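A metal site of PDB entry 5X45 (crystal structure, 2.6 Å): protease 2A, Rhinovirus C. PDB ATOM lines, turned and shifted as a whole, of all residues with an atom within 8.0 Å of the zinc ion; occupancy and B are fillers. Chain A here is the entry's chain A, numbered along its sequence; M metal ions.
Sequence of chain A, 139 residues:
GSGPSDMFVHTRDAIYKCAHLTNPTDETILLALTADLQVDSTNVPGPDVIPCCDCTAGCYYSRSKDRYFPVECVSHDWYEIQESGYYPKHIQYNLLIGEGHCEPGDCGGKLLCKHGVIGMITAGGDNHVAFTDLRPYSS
The guanidinium group of Arg 135 is in hydrogen-bond range of the backbone carbonyl oxygen of Cys 53 (3.4 Å). The side-chain sulfur of Cys 113 lies close to the backbone carbonyl oxygen of Gly 116 (3.7 Å). O of Cys 55 sits at hydrogen-bond distance from NH1 of Arg 135 (2.8 Å).
Within 4 Å of the zinc ion: Cys 53, Cys 55, Cys 113 and His 115. The nearest printed residue that does not touch the zinc ion is Lys 114 (4.5 Å).
The zinc ion is bound by SG of Cys 53 (1.9 Å), ND1 of His 115 (2.5 Å), SG of Cys 113 (2.5 Å) and SG of Cys 55 (2.6 Å).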
ATOM      1  N   PRO A  51      -7.349   3.691  14.988  1.00  0.00           N
ATOM      2  CA  PRO A  51      -6.284   4.668  14.805  1.00  0.00           C
ATOM      3  C   PRO A  51      -6.785   5.957  14.235  1.00  0.00           C
ATOM      4  O   PRO A  51      -7.836   5.991  13.665  1.00  0.00           O
ATOM      5  CB  PRO A  51      -5.365   3.987  13.801  1.00  0.00           C
ATOM      6  CG  PRO A  51      -6.163   2.932  13.165  1.00  0.00           C
ATOM      7  CD  PRO A  51      -7.363   2.663  13.947  1.00  0.00           C
ATOM      8  N   CYS A  52      -6.031   7.003  14.390  1.00  0.00           N
ATOM      9  CA  CYS A  52      -6.387   8.264  13.800  1.00  0.00           C
ATOM     10  C   CYS A  52      -5.475   8.482  12.640  1.00  0.00           C
ATOM     11  O   CYS A  52      -5.113   9.576  12.348  1.00  0.00           O
ATOM     12  CB  CYS A  52      -6.227   9.388  14.808  1.00  0.00           C
ATOM     13  SG  CYS A  52      -7.532   9.336  16.040  1.00  0.00           S
ATOM     14  N   CYS A  53      -5.093   7.414  11.992  1.00  0.00           N
ATOM     15  CA  CYS A  53      -4.272   7.508  10.829  1.00  0.00           C
ATOM     16  C   CYS A  53      -5.103   7.883   9.617  1.00  0.00           C
ATOM     17  O   CYS A  53      -6.274   8.189   9.701  1.00  0.00           O
ATOM     18  CB  CYS A  53      -3.419   6.226  10.630  1.00  0.00           C
ATOM     19  SG  CYS A  53      -4.154   4.641  10.149  1.00  0.00           S
ATOM     20  N   ASP A  54      -4.420   7.884   8.503  1.00  0.00           N
ATOM     21  CA  ASP A  54      -4.951   8.245   7.181  1.00  0.00           C
ATOM     22  C   ASP A  54      -4.969   7.069   6.198  1.00  0.00           C
ATOM     23  O   ASP A  54      -5.393   7.221   5.052  1.00  0.00           O
ATOM     24  CB  ASP A  54      -4.125   9.409   6.605  1.00  0.00           C
ATOM     25  CG  ASP A  54      -2.657   9.058   6.405  1.00  0.00           C
ATOM     26  OD1 ASP A  54      -2.070   8.373   7.286  1.00  0.00           O
ATOM     27  OD2 ASP A  54      -2.064   9.489   5.390  1.00  0.00           O
ATOM     28  N   CYS A  55      -4.497   5.905   6.652  1.00  0.00           N
ATOM     29  CA  CYS A  55      -4.376   4.724   5.791  1.00  0.00           C
ATOM     30  C   CYS A  55      -5.664   4.326   5.060  1.00  0.00           C
ATOM     31  O   CYS A  55      -6.776   4.517   5.560  1.00  0.00           O
ATOM     32  CB  CYS A  55      -3.894   3.524   6.608  1.00  0.00           C
ATOM     33  SG  CYS A  55      -2.200   3.678   7.204  1.00  0.00           S
ATOM     34  N   THR A  56      -5.484   3.795   3.849  1.00  0.00           N
ATOM     35  CA  THR A  56      -6.601   3.279   3.054  1.00  0.00           C
ATOM     36  C   THR A  56      -6.298   1.852   2.571  1.00  0.00           C
ATOM     37  O   THR A  56      -7.131   1.224   1.916  1.00  0.00           O
ATOM     38  CB  THR A  56      -6.873   4.182   1.822  1.00  0.00           C
ATOM     39  OG1 THR A  56      -5.641   4.462   1.138  1.00  0.00           O
ATOM     40  CG2 THR A  56      -7.543   5.491   2.246  1.00  0.00           C
ATOM     41  N   ALA A  57      -5.099   1.376   2.861  1.00  0.00           N
ATOM     42  CA  ALA A  57      -4.685   0.021   2.488  1.00  0.00           C
ATOM     43  C   ALA A  57      -4.417  -0.836   3.722  1.00  0.00           C
ATOM     44  O   ALA A  57      -3.878  -0.357   4.727  1.00  0.00           O
ATOM     45  CB  ALA A  57      -3.454   0.063   1.597  1.00  0.00           C
ATOM     46  N   LEU A 112      -8.202  -3.865   8.747  1.00  0.00           N
ATOM     47  CA  LEU A 112      -7.084  -3.399   9.549  1.00  0.00           C
ATOM     48  C   LEU A 112      -5.950  -2.797   8.733  1.00  0.00           C
ATOM     49  O   LEU A 112      -5.602  -3.302   7.671  1.00  0.00           O
ATOM     50  CB  LEU A 112      -6.506  -4.537  10.395  1.00  0.00           C
ATOM     51  CG  LEU A 112      -7.368  -5.111  11.510  1.00  0.00           C
ATOM     52  CD1 LEU A 112      -8.052  -6.368  11.018  1.00  0.00           C
ATOM     53  CD2 LEU A 112      -6.501  -5.382  12.721  1.00  0.00           C
ATOM     54  N   CYS A 113      -5.391  -1.719   9.241  1.00  0.00           N
ATOM     55  CA  CYS A 113      -4.104  -1.236   8.784  1.00  0.00           C
ATOM     56  C   CYS A 113      -3.050  -1.602   9.831  1.00  0.00           C
ATOM     57  O   CYS A 113      -3.350  -2.300  10.794  1.00  0.00           O
ATOM     58  CB  CYS A 113      -4.147   0.267   8.543  1.00  0.00           C
ATOM     59  SG  CYS A 113      -4.337   1.225  10.054  1.00  0.00           S
ATOM     60  N   LYS A 114      -1.834  -1.112   9.665  1.00  0.00           N
ATOM     61  CA  LYS A 114      -0.782  -1.421  10.613  1.00  0.00           C
ATOM     62  C   LYS A 114      -1.134  -0.923  12.027  1.00  0.00           C
ATOM     63  O   LYS A 114      -0.812  -1.570  13.016  1.00  0.00           O
ATOM     64  CB  LYS A 114       0.540  -0.801  10.137  1.00  0.00           C
ATOM     65  CG  LYS A 114       1.596  -0.699  11.213  1.00  0.00           C
ATOM     66  CD  LYS A 114       2.587   0.424  10.901  1.00  0.00           C
ATOM     67  CE  LYS A 114       3.524   0.617  12.065  1.00  0.00           C
ATOM     68  NZ  LYS A 114       4.165  -0.678  12.459  1.00  0.00           N
ATOM     69  N   HIS A 115      -1.816   0.218  12.103  1.00  0.00           N
ATOM     70  CA  HIS A 115      -2.084   0.873  13.382  1.00  0.00           C
ATOM     71  C   HIS A 115      -3.339   0.388  14.121  1.00  0.00           C
ATOM     72  O   HIS A 115      -3.511   0.657  15.305  1.00  0.00           O
ATOM     73  CB  HIS A 115      -2.154   2.382  13.173  1.00  0.00           C
ATOM     74  CG  HIS A 115      -0.919   2.948  12.534  1.00  0.00           C
ATOM     75  ND1 HIS A 115      -0.919   3.490  11.273  1.00  0.00           N
ATOM     76  CD2 HIS A 115       0.351   3.025  12.982  1.00  0.00           C
ATOM     77  CE1 HIS A 115       0.301   3.894  10.977  1.00  0.00           C
ATOM     78  NE2 HIS A 115       1.095   3.619  11.998  1.00  0.00           N
ATOM     79  N   GLY A 116      -4.211  -0.345  13.431  1.00  0.00           N
ATOM     80  CA  GLY A 116      -5.392  -0.892  14.074  1.00  0.00           C
ATOM     81  C   GLY A 116      -6.567  -1.105  13.136  1.00  0.00           C
ATOM     82  O   GLY A 116      -6.406  -1.199  11.931  1.00  0.00           O
ATOM     83  N   VAL A 117      -7.752  -1.213  13.719  1.00  0.00           N
ATOM     84  CA  VAL A 117      -8.966  -1.434  12.956  1.00  0.00           C
ATOM     85  C   VAL A 117      -9.528  -0.114  12.456  1.00  0.00           C
ATOM     86  O   VAL A 117      -9.787   0.801  13.244  1.00  0.00           O
ATOM     87  CB  VAL A 117     -10.019  -2.148  13.803  1.00  0.00           C
ATOM     88  CG1 VAL A 117     -11.197  -2.578  12.920  1.00  0.00           C
ATOM     89  CG2 VAL A 117      -9.410  -3.370  14.492  1.00  0.00           C
ATOM     90  N   ILE A 118      -9.735   0.012  11.146  1.00  0.00           N
ATOM     91  CA  ILE A 118     -10.247   1.265  10.600  1.00  0.00           C
ATOM     92  C   ILE A 118     -11.626   1.089   9.967  1.00  0.00           C
ATOM     93  O   ILE A 118     -12.260   2.073   9.612  1.00  0.00           O
ATOM     94  CB  ILE A 118      -9.289   1.854   9.534  1.00  0.00           C
ATOM     95  CG1 ILE A 118      -9.120   0.897   8.362  1.00  0.00           C
ATOM     96  CG2 ILE A 118      -7.946   2.231  10.139  1.00  0.00           C
ATOM     97  CD1 ILE A 118      -8.263   1.435   7.249  1.00  0.00           C
ATOM     98  N   ARG A 135     -13.215   5.550  11.636  1.00  0.00           N
ATOM     99  CA  ARG A 135     -12.491   6.709  12.156  1.00  0.00           C
ATOM    100  C   ARG A 135     -13.349   7.963  12.362  1.00  0.00           C
ATOM    101  O   ARG A 135     -13.216   8.617  13.404  1.00  0.00           O
ATOM    102  CB  ARG A 135     -11.283   7.008  11.261  1.00  0.00           C
ATOM    103  CG  ARG A 135     -10.203   5.932  11.354  1.00  0.00           C
ATOM    104  CD  ARG A 135      -9.144   6.092  10.287  1.00  0.00           C
ATOM    105  NE  ARG A 135      -9.693   5.844   8.960  1.00  0.00           N
ATOM    106  CZ  ARG A 135      -8.964   5.634   7.870  1.00  0.00           C
ATOM    107  NH1 ARG A 135      -7.639   5.621   7.950  1.00  0.00           N
ATOM    108  NH2 ARG A 135      -9.555   5.408   6.708  1.00  0.00           N
HETATM  109 ZN    ZN M   1      -2.855   3.265   9.732  1.00  0.00          ZN
